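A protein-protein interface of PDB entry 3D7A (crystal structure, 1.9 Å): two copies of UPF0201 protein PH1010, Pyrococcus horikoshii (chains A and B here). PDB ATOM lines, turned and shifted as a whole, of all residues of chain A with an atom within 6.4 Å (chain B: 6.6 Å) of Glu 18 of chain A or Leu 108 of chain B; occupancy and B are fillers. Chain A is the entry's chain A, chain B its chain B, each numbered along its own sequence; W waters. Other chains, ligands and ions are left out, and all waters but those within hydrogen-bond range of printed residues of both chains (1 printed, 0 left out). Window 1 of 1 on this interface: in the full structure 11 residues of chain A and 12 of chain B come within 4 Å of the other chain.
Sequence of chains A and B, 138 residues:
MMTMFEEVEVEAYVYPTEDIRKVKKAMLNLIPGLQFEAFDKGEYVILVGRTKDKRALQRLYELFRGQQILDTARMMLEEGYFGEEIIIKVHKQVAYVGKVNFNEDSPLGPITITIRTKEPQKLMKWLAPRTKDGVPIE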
ATOM      1  N   TYR A  13      -9.136  -7.795  19.240  1.00  0.00           N
ATOM      2  CA  TYR A  13      -7.885  -7.120  19.526  1.00  0.00           C
ATOM      3  C   TYR A  13      -7.651  -6.119  18.413  1.00  0.00           C
ATOM      4  O   TYR A  13      -7.957  -6.404  17.245  1.00  0.00           O
ATOM      5  CB  TYR A  13      -6.753  -8.136  19.526  1.00  0.00           C
ATOM      6  CG  TYR A  13      -6.689  -8.999  20.760  1.00  0.00           C
ATOM      7  CD1 TYR A  13      -7.711  -8.981  21.705  1.00  0.00           C
ATOM      8  CD2 TYR A  13      -5.599  -9.823  20.991  1.00  0.00           C
ATOM      9  CE1 TYR A  13      -7.649  -9.781  22.857  1.00  0.00           C
ATOM     10  CE2 TYR A  13      -5.539 -10.633  22.126  1.00  0.00           C
ATOM     11  CZ  TYR A  13      -6.559 -10.603  23.052  1.00  0.00           C
ATOM     12  OH  TYR A  13      -6.491 -11.409  24.185  1.00  0.00           O
ATOM     13  N   VAL A  14      -7.130  -4.957  18.785  1.00  0.00           N
ATOM     14  CA  VAL A  14      -6.794  -3.900  17.842  1.00  0.00           C
ATOM     15  C   VAL A  14      -5.281  -3.699  17.912  1.00  0.00           C
ATOM     16  O   VAL A  14      -4.745  -3.195  18.932  1.00  0.00           O
ATOM     17  CB  VAL A  14      -7.526  -2.587  18.155  1.00  0.00           C
ATOM     18  CG1 VAL A  14      -7.284  -1.561  17.040  1.00  0.00           C
ATOM     19  CG2 VAL A  14      -9.040  -2.799  18.306  1.00  0.00           C
ATOM     20  N   TYR A  15      -4.585  -4.103  16.855  1.00  0.00           N
ATOM     21  CA  TYR A  15      -3.131  -4.005  16.859  1.00  0.00           C
ATOM     22  C   TYR A  15      -2.657  -2.612  16.465  1.00  0.00           C
ATOM     23  O   TYR A  15      -3.423  -1.829  15.912  1.00  0.00           O
ATOM     24  CB  TYR A  15      -2.515  -5.121  16.008  1.00  0.00           C
ATOM     25  CG  TYR A  15      -2.756  -6.482  16.640  1.00  0.00           C
ATOM     26  CD1 TYR A  15      -3.825  -7.294  16.227  1.00  0.00           C
ATOM     27  CD2 TYR A  15      -1.938  -6.938  17.675  1.00  0.00           C
ATOM     28  CE1 TYR A  15      -4.059  -8.545  16.821  1.00  0.00           C
ATOM     29  CE2 TYR A  15      -2.152  -8.172  18.275  1.00  0.00           C
ATOM     30  CZ  TYR A  15      -3.209  -8.978  17.841  1.00  0.00           C
ATOM     31  OH  TYR A  15      -3.427 -10.196  18.442  1.00  0.00           O
ATOM     32  N   PRO A  16      -1.394  -2.285  16.803  1.00  0.00           N
ATOM     33  CA  PRO A  16      -0.837  -0.989  16.519  1.00  0.00           C
ATOM     34  C   PRO A  16      -1.008  -0.554  15.066  1.00  0.00           C
ATOM     35  O   PRO A  16      -1.331   0.594  14.847  1.00  0.00           O
ATOM     36  CB  PRO A  16       0.645  -1.158  16.888  1.00  0.00           C
ATOM     37  CG  PRO A  16       0.605  -2.118  18.072  1.00  0.00           C
ATOM     38  CD  PRO A  16      -0.495  -3.116  17.629  1.00  0.00           C
ATOM     39  N   THR A  17      -0.818  -1.438  14.082  1.00  0.00           N
ATOM     40  CA  THR A  17      -1.041  -1.026  12.682  1.00  0.00           C
ATOM     41  C   THR A  17      -2.509  -0.982  12.291  1.00  0.00           C
ATOM     42  O   THR A  17      -2.859  -0.520  11.193  1.00  0.00           O
ATOM     43  CB  THR A  17      -0.300  -1.902  11.683  1.00  0.00           C
ATOM     44  OG1 THR A  17      -0.760  -3.266  11.816  1.00  0.00           O
ATOM     45  CG2 THR A  17       1.198  -1.791  11.918  1.00  0.00           C
ATOM     46  N   GLU A  18      -3.377  -1.397  13.204  1.00  0.00           N
ATOM     47  CA  GLU A  18      -4.801  -1.285  12.940  1.00  0.00           C
ATOM     48  C   GLU A  18      -5.396   0.056  13.324  1.00  0.00           C
ATOM     49  O   GLU A  18      -4.863   0.776  14.164  1.00  0.00           O
ATOM     50  CB  GLU A  18      -5.589  -2.406  13.607  1.00  0.00           C
ATOM     51  CG  GLU A  18      -5.405  -3.732  12.908  1.00  0.00           C
ATOM     52  CD  GLU A  18      -6.214  -4.828  13.551  1.00  0.00           C
ATOM     53  OE1 GLU A  18      -5.914  -5.153  14.704  1.00  0.00           O
ATOM     54  OE2 GLU A  18      -7.145  -5.376  12.903  1.00  0.00           O
ATOM     55  N   ASP A  19      -6.541   0.337  12.713  1.00  0.00           N
ATOM     56  CA  ASP A  19      -7.413   1.474  12.985  1.00  0.00           C
ATOM     57  C   ASP A  19      -8.512   1.041  13.967  1.00  0.00           C
ATOM     58  O   ASP A  19      -9.269   0.119  13.653  1.00  0.00           O
ATOM     59  CB  ASP A  19      -8.071   1.766  11.644  1.00  0.00           C
ATOM     60  CG  ASP A  19      -8.203   3.213  11.349  1.00  0.00           C
ATOM     61  OD1 ASP A  19      -9.091   3.860  11.955  1.00  0.00           O
ATOM     62  OD2 ASP A  19      -7.445   3.681  10.460  1.00  0.00           O
ATOM     63  N   ILE A  20      -8.613   1.642  15.152  1.00  0.00           N
ATOM     64  CA  ILE A  20      -9.619   1.158  16.135  1.00  0.00           C
ATOM     65  C   ILE A  20     -11.026   1.321  15.546  1.00  0.00           C
ATOM     66  O   ILE A  20     -11.870   0.455  15.707  1.00  0.00           O
ATOM     67  CB  ILE A  20      -9.530   1.860  17.521  1.00  0.00           C
ATOM     68  CG1 ILE A  20     -10.332   1.066  18.575  1.00  0.00           C
ATOM     69  CG2 ILE A  20      -9.992   3.316  17.403  1.00  0.00           C
ATOM     70  CD1 ILE A  20     -10.065   1.454  20.061  1.00  0.00           C
ATOM     71  N   LYS A  22     -11.931   1.061  12.366  1.00  0.00           N
ATOM     72  CA  LYS A  22     -12.236   0.031  11.381  1.00  0.00           C
ATOM     73  C   LYS A  22     -12.623  -1.275  12.106  1.00  0.00           C
ATOM     74  O   LYS A  22     -13.531  -1.993  11.686  1.00  0.00           O
ATOM     75  CB  LYS A  22     -11.027  -0.194  10.449  1.00  0.00           C
ATOM     76  CG  LYS A  22     -10.873   0.914   9.390  1.00  0.00           C
ATOM     77  CD  LYS A  22      -9.659   0.640   8.534  1.00  0.00           C
ATOM     78  CE  LYS A  22      -9.476   1.755   7.504  1.00  0.00           C
ATOM     79  NZ  LYS A  22      -8.262   1.557   6.712  1.00  0.00           N
ATOM     80  N   VAL A  23     -11.942  -1.590  13.202  1.00  0.00           N
ATOM     81  CA  VAL A  23     -12.314  -2.798  13.944  1.00  0.00           C
ATOM     82  C   VAL A  23     -13.703  -2.657  14.587  1.00  0.00           C
ATOM     83  O   VAL A  23     -14.493  -3.594  14.581  1.00  0.00           O
ATOM     84  CB  VAL A  23     -11.227  -3.215  14.984  1.00  0.00           C
ATOM     85  CG1 VAL A  23     -11.652  -4.463  15.723  1.00  0.00           C
ATOM     86  CG2 VAL A  23      -9.885  -3.451  14.295  1.00  0.00           C
ATOM     87  N   LYS A  92     -12.127 -11.580  11.077  1.00  0.00           N
ATOM     88  CA  LYS A  92     -12.182 -10.153  11.288  1.00  0.00           C
ATOM     89  C   LYS A  92     -12.293  -9.417   9.939  1.00  0.00           C
ATOM     90  O   LYS A  92     -13.067  -8.485   9.829  1.00  0.00           O
ATOM     91  CB  LYS A  92     -10.927  -9.648  12.006  1.00  0.00           C
ATOM     92  CG  LYS A  92     -10.973  -8.150  12.333  1.00  0.00           C
ATOM     93  CD  LYS A  92      -9.620  -7.628  12.824  1.00  0.00           C
ATOM     94  CE  LYS A  92      -9.536  -7.559  14.330  1.00  0.00           C
ATOM     95  NZ  LYS A  92      -8.112  -7.183  14.678  1.00  0.00           N
ATOM     96  N   GLN A  93     -11.505  -9.818   8.960  1.00  0.00           N
ATOM     97  CA  GLN A  93     -11.443  -9.067   7.691  1.00  0.00           C
ATOM     98  C   GLN A  93     -12.722  -9.283   6.882  1.00  0.00           C
ATOM     99  O   GLN A  93     -13.205  -8.353   6.210  1.00  0.00           O
ATOM    100  CB  GLN A  93     -10.193  -9.428   6.870  1.00  0.00           C
ATOM    101  CG  GLN A  93      -8.848  -9.242   7.610  1.00  0.00           C
ATOM    102  CD  GLN A  93      -8.707  -7.845   8.236  1.00  0.00           C
ATOM    103  OE1 GLN A  93      -9.071  -6.842   7.636  1.00  0.00           O
ATOM    104  NE2 GLN A  93      -8.216  -7.794   9.458  1.00  0.00           N
ATOM    105  N   SER A 106      -7.691 -15.903  11.082  1.00  0.00           N
ATOM    106  CA  SER A 106      -8.017 -14.519  10.775  1.00  0.00           C
ATOM    107  C   SER A 106      -6.785 -13.574  10.904  1.00  0.00           C
ATOM    108  O   SER A 106      -6.184 -13.465  11.977  1.00  0.00           O
ATOM    109  CB  SER A 106      -9.201 -14.091  11.680  1.00  0.00           C
ATOM    110  OG  SER A 106      -9.522 -12.711  11.616  1.00  0.00           O
ATOM    111  N   PRO A 107      -6.395 -12.910   9.789  1.00  0.00           N
ATOM    112  CA  PRO A 107      -5.357 -11.874   9.855  1.00  0.00           C
ATOM    113  C   PRO A 107      -5.691 -10.918  10.999  1.00  0.00           C
ATOM    114  O   PRO A 107      -6.803 -10.337  11.058  1.00  0.00           O
ATOM    115  CB  PRO A 107      -5.450 -11.201   8.492  1.00  0.00           C
ATOM    116  CG  PRO A 107      -5.942 -12.317   7.602  1.00  0.00           C
ATOM    117  CD  PRO A 107      -6.968 -13.001   8.433  1.00  0.00           C
ATOM    118  N   LEU A 108      -4.647 -10.664  11.787  1.00  0.00           N
ATOM    119  CA  LEU A 108      -4.640 -11.095  13.168  1.00  0.00           C
ATOM    120  C   LEU A 108      -5.860 -10.922  14.007  1.00  0.00           C
ATOM    121  O   LEU A 108      -6.406  -9.823  14.171  1.00  0.00           O
ATOM    122  CB  LEU A 108      -3.388 -10.715  13.929  1.00  0.00           C
ATOM    123  CG  LEU A 108      -2.479 -11.900  14.336  1.00  0.00           C
ATOM    124  CD1 LEU A 108      -3.088 -12.736  15.495  1.00  0.00           C
ATOM    125  CD2 LEU A 108      -2.110 -12.796  13.122  1.00  0.00           C
ATOM    126  N   GLY A 109      -6.259 -12.060  14.559  1.00  0.00           N
ATOM    127  CA  GLY A 109      -7.258 -12.074  15.578  1.00  0.00           C
ATOM    128  C   GLY A 109      -8.604 -12.281  14.929  1.00  0.00           C
ATOM    129  O   GLY A 109      -8.929 -11.632  13.936  1.00  0.00           O
ATOM    130  N   ALA B  12       5.302  -5.812   3.059  1.00  0.00           N
ATOM    131  CA  ALA B  12       4.301  -6.100   4.095  1.00  0.00           C
ATOM    132  C   ALA B  12       2.896  -6.107   3.474  1.00  0.00           C
ATOM    133  O   ALA B  12       2.661  -5.457   2.448  1.00  0.00           O
ATOM    134  CB  ALA B  12       4.367  -5.064   5.212  1.00  0.00           C
ATOM    135  N   TYR B  13       1.976  -6.854   4.066  1.00  0.00           N
ATOM    136  CA  TYR B  13       0.587  -6.798   3.636  1.00  0.00           C
ATOM    137  C   TYR B  13      -0.134  -5.744   4.444  1.00  0.00           C
ATOM    138  O   TYR B  13       0.206  -5.478   5.631  1.00  0.00           O
ATOM    139  CB  TYR B  13      -0.104  -8.169   3.734  1.00  0.00           C
ATOM    140  CG  TYR B  13       0.410  -9.232   2.776  1.00  0.00           C
ATOM    141  CD1 TYR B  13       1.307  -8.926   1.763  1.00  0.00           C
ATOM    142  CD2 TYR B  13      -0.027 -10.541   2.871  1.00  0.00           C
ATOM    143  CE1 TYR B  13       1.774  -9.896   0.908  1.00  0.00           C
ATOM    144  CE2 TYR B  13       0.422 -11.517   2.006  1.00  0.00           C
ATOM    145  CZ  TYR B  13       1.325 -11.190   1.028  1.00  0.00           C
ATOM    146  OH  TYR B  13       1.782 -12.165   0.170  1.00  0.00           O
ATOM    147  N   VAL B  14      -1.076  -5.070   3.788  1.00  0.00           N
ATOM    148  CA  VAL B  14      -1.981  -4.187   4.491  1.00  0.00           C
ATOM    149  C   VAL B  14      -3.373  -4.777   4.402  1.00  0.00           C
ATOM    150  O   VAL B  14      -3.980  -4.809   3.315  1.00  0.00           O
ATOM    151  CB  VAL B  14      -1.979  -2.741   3.919  1.00  0.00           C
ATOM    152  CG1 VAL B  14      -2.780  -1.781   4.841  1.00  0.00           C
ATOM    153  CG2 VAL B  14      -0.526  -2.266   3.716  1.00  0.00           C
ATOM    154  N   TYR B  15      -3.897  -5.206   5.551  1.00  0.00           N
ATOM    155  CA  TYR B  15      -5.254  -5.764   5.600  1.00  0.00           C
ATOM    156  C   TYR B  15      -6.278  -4.666   5.713  1.00  0.00           C
ATOM    157  O   TYR B  15      -5.946  -3.540   6.086  1.00  0.00           O
ATOM    158  CB  TYR B  15      -5.359  -6.762   6.783  1.00  0.00           C
ATOM    159  CG  TYR B  15      -4.601  -8.023   6.478  1.00  0.00           C
ATOM    160  CD1 TYR B  15      -3.309  -8.232   6.962  1.00  0.00           C
ATOM    161  CD2 TYR B  15      -5.151  -8.992   5.631  1.00  0.00           C
ATOM    162  CE1 TYR B  15      -2.614  -9.385   6.634  1.00  0.00           C
ATOM    163  CE2 TYR B  15      -4.466 -10.132   5.320  1.00  0.00           C
ATOM    164  CZ  TYR B  15      -3.209 -10.333   5.832  1.00  0.00           C
ATOM    165  OH  TYR B  15      -2.549 -11.489   5.498  1.00  0.00           O
ATOM    166  N   PRO B  16      -7.547  -4.973   5.383  1.00  0.00           N
ATOM    167  CA  PRO B  16      -8.569  -3.927   5.429  1.00  0.00           C
ATOM    168  C   PRO B  16      -8.736  -3.215   6.776  1.00  0.00           C
ATOM    169  O   PRO B  16      -9.143  -2.056   6.782  1.00  0.00           O
ATOM    170  CB  PRO B  16      -9.865  -4.675   5.036  1.00  0.00           C
ATOM    171  CG  PRO B  16      -9.409  -5.804   4.185  1.00  0.00           C
ATOM    172  CD  PRO B  16      -8.031  -6.214   4.752  1.00  0.00           C
ATOM    173  N   THR B  17      -8.451  -3.865   7.914  1.00  0.00           N
ATOM    174  CA  THR B  17      -8.609  -3.146   9.180  1.00  0.00           C
ATOM    175  C   THR B  17      -7.346  -2.342   9.567  1.00  0.00           C
ATOM    176  O   THR B  17      -7.327  -1.656  10.605  1.00  0.00           O
ATOM    177  CB  THR B  17      -8.994  -4.077  10.355  1.00  0.00           C
ATOM    178  OG1 THR B  17      -7.981  -5.051  10.539  1.00  0.00           O
ATOM    179  CG2 THR B  17     -10.326  -4.790  10.107  1.00  0.00           C
ATOM    180  N   GLU B  18      -6.313  -2.438   8.733  1.00  0.00           N
ATOM    181  CA  GLU B  18      -5.075  -1.669   8.913  1.00  0.00           C
ATOM    182  C   GLU B  18      -5.070  -0.308   8.203  1.00  0.00           C
ATOM    183  O   GLU B  18      -5.850  -0.067   7.275  1.00  0.00           O
ATOM    184  CB  GLU B  18      -3.895  -2.490   8.405  1.00  0.00           C
ATOM    185  CG  GLU B  18      -3.584  -3.725   9.247  1.00  0.00           C
ATOM    186  CD  GLU B  18      -2.318  -4.404   8.808  1.00  0.00           C
ATOM    187  OE1 GLU B  18      -2.318  -5.107   7.768  1.00  0.00           O
ATOM    188  OE2 GLU B  18      -1.283  -4.250   9.519  1.00  0.00           O
ATOM    189  N   ASP B  19      -4.183   0.583   8.657  1.00  0.00           N
ATOM    190  CA  ASP B  19      -3.923   1.858   7.988  1.00  0.00           C
ATOM    191  C   ASP B  19      -2.600   1.694   7.249  1.00  0.00           C
ATOM    192  O   ASP B  19      -1.551   1.460   7.860  1.00  0.00           O
ATOM    193  CB  ASP B  19      -3.873   2.979   9.035  1.00  0.00           C
ATOM    194  CG  ASP B  19      -3.562   4.333   8.449  1.00  0.00           C
ATOM    195  OD1 ASP B  19      -3.265   4.433   7.231  1.00  0.00           O
ATOM    196  OD2 ASP B  19      -3.611   5.305   9.223  1.00  0.00           O
ATOM    197  N   LYS B  22       0.278   3.513   8.724  1.00  0.00           N
ATOM    198  CA  LYS B  22       0.919   2.861   9.888  1.00  0.00           C
ATOM    199  C   LYS B  22       1.881   1.746   9.505  1.00  0.00           C
ATOM    200  O   LYS B  22       2.948   1.592  10.127  1.00  0.00           O
ATOM    201  CB  LYS B  22      -0.139   2.361  10.864  1.00  0.00           C
ATOM    202  CG  LYS B  22      -0.950   3.459  11.519  1.00  0.00           C
ATOM    203  CD  LYS B  22      -1.966   2.864  12.491  1.00  0.00           C
ATOM    204  CE  LYS B  22      -2.771   3.935  13.248  1.00  0.00           C
ATOM    205  NZ  LYS B  22      -3.778   3.342  14.187  1.00  0.00           N
ATOM    206  N   LYS B  92       5.714  -7.092  12.662  1.00  0.00           N
ATOM    207  CA  LYS B  92       5.234  -5.813  12.116  1.00  0.00           C
ATOM    208  C   LYS B  92       4.888  -4.806  13.215  1.00  0.00           C
ATOM    209  O   LYS B  92       5.177  -3.608  13.118  1.00  0.00           O
ATOM    210  CB  LYS B  92       3.972  -6.071  11.236  1.00  0.00           C
ATOM    211  CG  LYS B  92       3.330  -4.778  10.695  1.00  0.00           C
ATOM    212  CD  LYS B  92       1.922  -5.022  10.125  1.00  0.00           C
ATOM    213  CE  LYS B  92       1.990  -5.893   8.872  1.00  0.00           C
ATOM    214  NZ  LYS B  92       0.631  -6.020   8.241  1.00  0.00           N
ATOM    215  N   GLN B  93       4.250  -5.312  14.262  1.00  0.00           N
ATOM    216  CA  GLN B  93       3.795  -4.482  15.377  1.00  0.00           C
ATOM    217  C   GLN B  93       4.982  -4.006  16.220  1.00  0.00           C
ATOM    218  O   GLN B  93       4.965  -2.889  16.709  1.00  0.00           O
ATOM    219  CB  GLN B  93       2.752  -5.234  16.235  1.00  0.00           C
ATOM    220  CG  GLN B  93       1.693  -5.941  15.351  1.00  0.00           C
ATOM    221  CD  GLN B  93       0.920  -4.949  14.463  1.00  0.00           C
ATOM    222  OE1 GLN B  93       0.710  -3.815  14.844  1.00  0.00           O
ATOM    223  NE2 GLN B  93       0.490  -5.397  13.282  1.00  0.00           N
ATOM    224  N   SER B 106       3.516 -12.890  13.781  1.00  0.00           N
ATOM    225  CA  SER B 106       3.371 -11.445  13.776  1.00  0.00           C
ATOM    226  C   SER B 106       1.930 -11.105  13.447  1.00  0.00           C
ATOM    227  O   SER B 106       1.437 -11.460  12.373  1.00  0.00           O
ATOM    228  CB  SER B 106       4.305 -10.822  12.729  1.00  0.00           C
ATOM    229  OG  SER B 106       4.002  -9.456  12.501  1.00  0.00           O
ATOM    230  N   PRO B 107       1.240 -10.442  14.391  1.00  0.00           N
ATOM    231  CA  PRO B 107      -0.066  -9.891  14.108  1.00  0.00           C
ATOM    232  C   PRO B 107      -0.145  -9.158  12.752  1.00  0.00           C
ATOM    233  O   PRO B 107       0.596  -8.171  12.478  1.00  0.00           O
ATOM    234  CB  PRO B 107      -0.301  -8.961  15.294  1.00  0.00           C
ATOM    235  CG  PRO B 107       0.340  -9.724  16.437  1.00  0.00           C
ATOM    236  CD  PRO B 107       1.594 -10.309  15.819  1.00  0.00           C
ATOM    237  N   LEU B 108      -1.045  -9.688  11.919  1.00  0.00           N
ATOM    238  CA  LEU B 108      -1.313  -9.194  10.567  1.00  0.00           C
ATOM    239  C   LEU B 108      -0.112  -9.380   9.648  1.00  0.00           C
ATOM    240  O   LEU B 108       0.135  -8.578   8.749  1.00  0.00           O
ATOM    241  CB  LEU B 108      -1.861  -7.748  10.586  1.00  0.00           C
ATOM    242  CG  LEU B 108      -3.328  -7.691  11.067  1.00  0.00           C
ATOM    243  CD1 LEU B 108      -3.449  -6.768  12.265  1.00  0.00           C
ATOM    244  CD2 LEU B 108      -4.310  -7.397   9.921  1.00  0.00           C
ATOM    245  N   GLY B 109       0.600 -10.493   9.865  1.00  0.00           N
ATOM    246  CA  GLY B 109       1.736 -10.911   9.030  1.00  0.00           C
ATOM    247  C   GLY B 109       3.033 -10.177   9.339  1.00  0.00           C
ATOM    248  O   GLY B 109       3.008  -9.103   9.945  1.00  0.00           O
ATOM    249  N   PRO B 110       4.180 -10.758   8.937  1.00  0.00           N
ATOM    250  CA  PRO B 110       5.453 -10.101   9.214  1.00  0.00           C
ATOM    251  C   PRO B 110       5.785  -9.006   8.207  1.00  0.00           C
ATOM    252  O   PRO B 110       5.083  -8.843   7.213  1.00  0.00           O
ATOM    253  CB  PRO B 110       6.471 -11.223   9.043  1.00  0.00           C
ATOM    254  CG  PRO B 110       5.829 -12.179   8.063  1.00  0.00           C
ATOM    255  CD  PRO B 110       4.357 -12.116   8.376  1.00  0.00           C
HETATM  256  O   HOH W   1      -5.391   5.778  11.221  1.00  0.00           O
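Water W1 bridges OD2 of Asp 19 of chain B (2.7 Å) and OD2 of Asp 19 of chain A (3.0 Å).
Gln 93 of chain B touches Tyr 15 of chain A (OE1 to CB, 3.7 Å). Pro 107 of chain B touches Tyr 15 of chain A. Asp 19 of chain B touches Asp 19 of chain A. Lys 22 of chain A touches Pro 16 of chain B (CD to O, 3.3 Å). Thr 17 of chain B touches Lys 22 of chain A (O to CD, 3.9 Å). Lys 92 of chain A touches Thr 17 of chain B (CD to OG1, 3.8 Å). Gln 93 of chain A touches Leu 108 of chain B. Pro 107 of chain A touches Leu 108 of chain B. CA of Pro 107 of chain B touches CG of Leu 108 of chain A, 3.1 Å away. Leu 108 of chain A touches Leu 108 of chain B.
OE2 of Glu 18 of chain B sits at hydrogen-bond distance from OG1 of Thr 17 of chain A, 2.6 Å away. O of Thr 17 of chain A is in hydrogen-bond range of N of Asp 19 of chain B, at 3.1 Å. OG1 of Thr 17 of chain A lies within hydrogen-bond range of NE2 of Gln 93 of chain B, at 2.9 Å. OE2 of Glu 18 of chain A sits at hydrogen-bond distance from OG1 of Thr 17 of chain B (2.5 Å). The backbone carbonyl oxygen (O) of Glu 18 of chain A is in hydrogen-bond range of the side-chain amino group (NZ) of Lys 22 of chain B (2.8 Å). N of Asp 19 of chain A is in hydrogen-bond range of O of Thr 17 of chain B (3.0 Å). The side-chain amino group (NZ) of Lys 22 of chain A is in hydrogen-bond range of the backbone carbonyl oxygen (O) of Glu 18 of chain B (3.0 Å). The side-chain amide nitrogen (NE2) of Gln 93 of chain A is in hydrogen-bond range of the side-chain hydroxyl (OG1) of Thr 17 of chain B (3.0 Å). N of Pro 16 of chain A lies close to OE1 of Gln 93 of chain B (3.3 Å). The side-chain amide oxygen (OE1) of Gln 93 of chain A sits close to the backbone nitrogen (N) of Pro 16 of chain B (3.3 Å).
Of the 16 printed residues of chain A, 10 touch a printed residue of chain B. Printed residues of chain B that touch a printed residue of chain A: Tyr 15, Pro 16, Thr 17, Glu 18, Asp 19, Lys 22, Lys 92, Gln 93, Ser 106, Pro 107 and Leu 108. Hydrophobic or aromatic side chains of chain B that line the printed part of chain A: Tyr 15, Pro 16, Pro 107 and Leu 108. Among the printed residues, no Asp or Glu carboxylate lies within 4 Å of a Lys or Arg side-chain nitrogen of the other chain.
Of the printed residues of chain B, Thr 17 of chain A touches Glu 18, Asp 19, Lys 22, Lys 92 and Gln 93. Of chain B, only Thr 17, Lys 22 and Leu 108 come within 4 Å of Glu 18 of chain A. Of the printed residues of chain A, Lys 92 of chain B touches Thr 17 (3.6 Å). Of the printed residues of chain A, Leu 108 of chain B touches Glu 18, Gln 93, Pro 107 and Leu 108. The nearest residue of chain B that does not touch Glu 18 of chain A is Glu 18 of chain B (4.1 Å). The nearest printed residue of chain B that does not touch Asp 19 of chain A is Lys 22 of chain B (4.3 Å).
The backbone NH of Lys 92 of chain A sits at hydrogen-bond distance from the side-chain hydroxyl of Ser 106 of chain A (2.9 Å). The side-chain amino group of Lys 92 of chain A sits at hydrogen-bond distance from the backbone carbonyl oxygen of Leu 108 of chain A, at 3.2 Å. The side-chain amide nitrogen (NE2) of Gln 93 of chain A is in hydrogen-bond range of the backbone carbonyl oxygen (O) of Pro 107 of chain A (3.3 Å). The backbone carbonyl oxygen (O) of Tyr 13 of chain B sits at hydrogen-bond distance from the side-chain amino group (NZ) of Lys 92 of chain B. The backbone NH (N) of Lys 92 of chain B lies within hydrogen-bond range of the side-chain hydroxyl (OG) of Ser 106 of chain B (2.9 Å). O of Pro 107 of chain B is in hydrogen-bond range of NE2 of Gln 93 of chain B, 2.9 Å away.
Pro 16 of chain A touches Lys 22 of chain B, and with the chains exchanged Lys 22 of chain A touches Pro 16 of chain B. Thr 17 of chain A touches Lys 22 of chain B, and with the chains exchanged Lys 22 of chain A touches Thr 17 of chain B. Thr 17 of chain A touches Gln 93 of chain B, and with the chains exchanged Gln 93 of chain A touches Thr 17 of chain B. Glu 18 of chain A touches Leu 108 of chain B, but with the chains exchanged Leu 108 of chain A does not touch Glu 18 of chain B (7.2 Å). Positions printed for both chains: 13, 14, 15, 16, 17, 18, 19, 22, 92, 93, 106, 107, 108 and 109. Of the 27 pairs that touch across the chains among the printed residues, 24 have their exchanged pair printed and touching as well.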
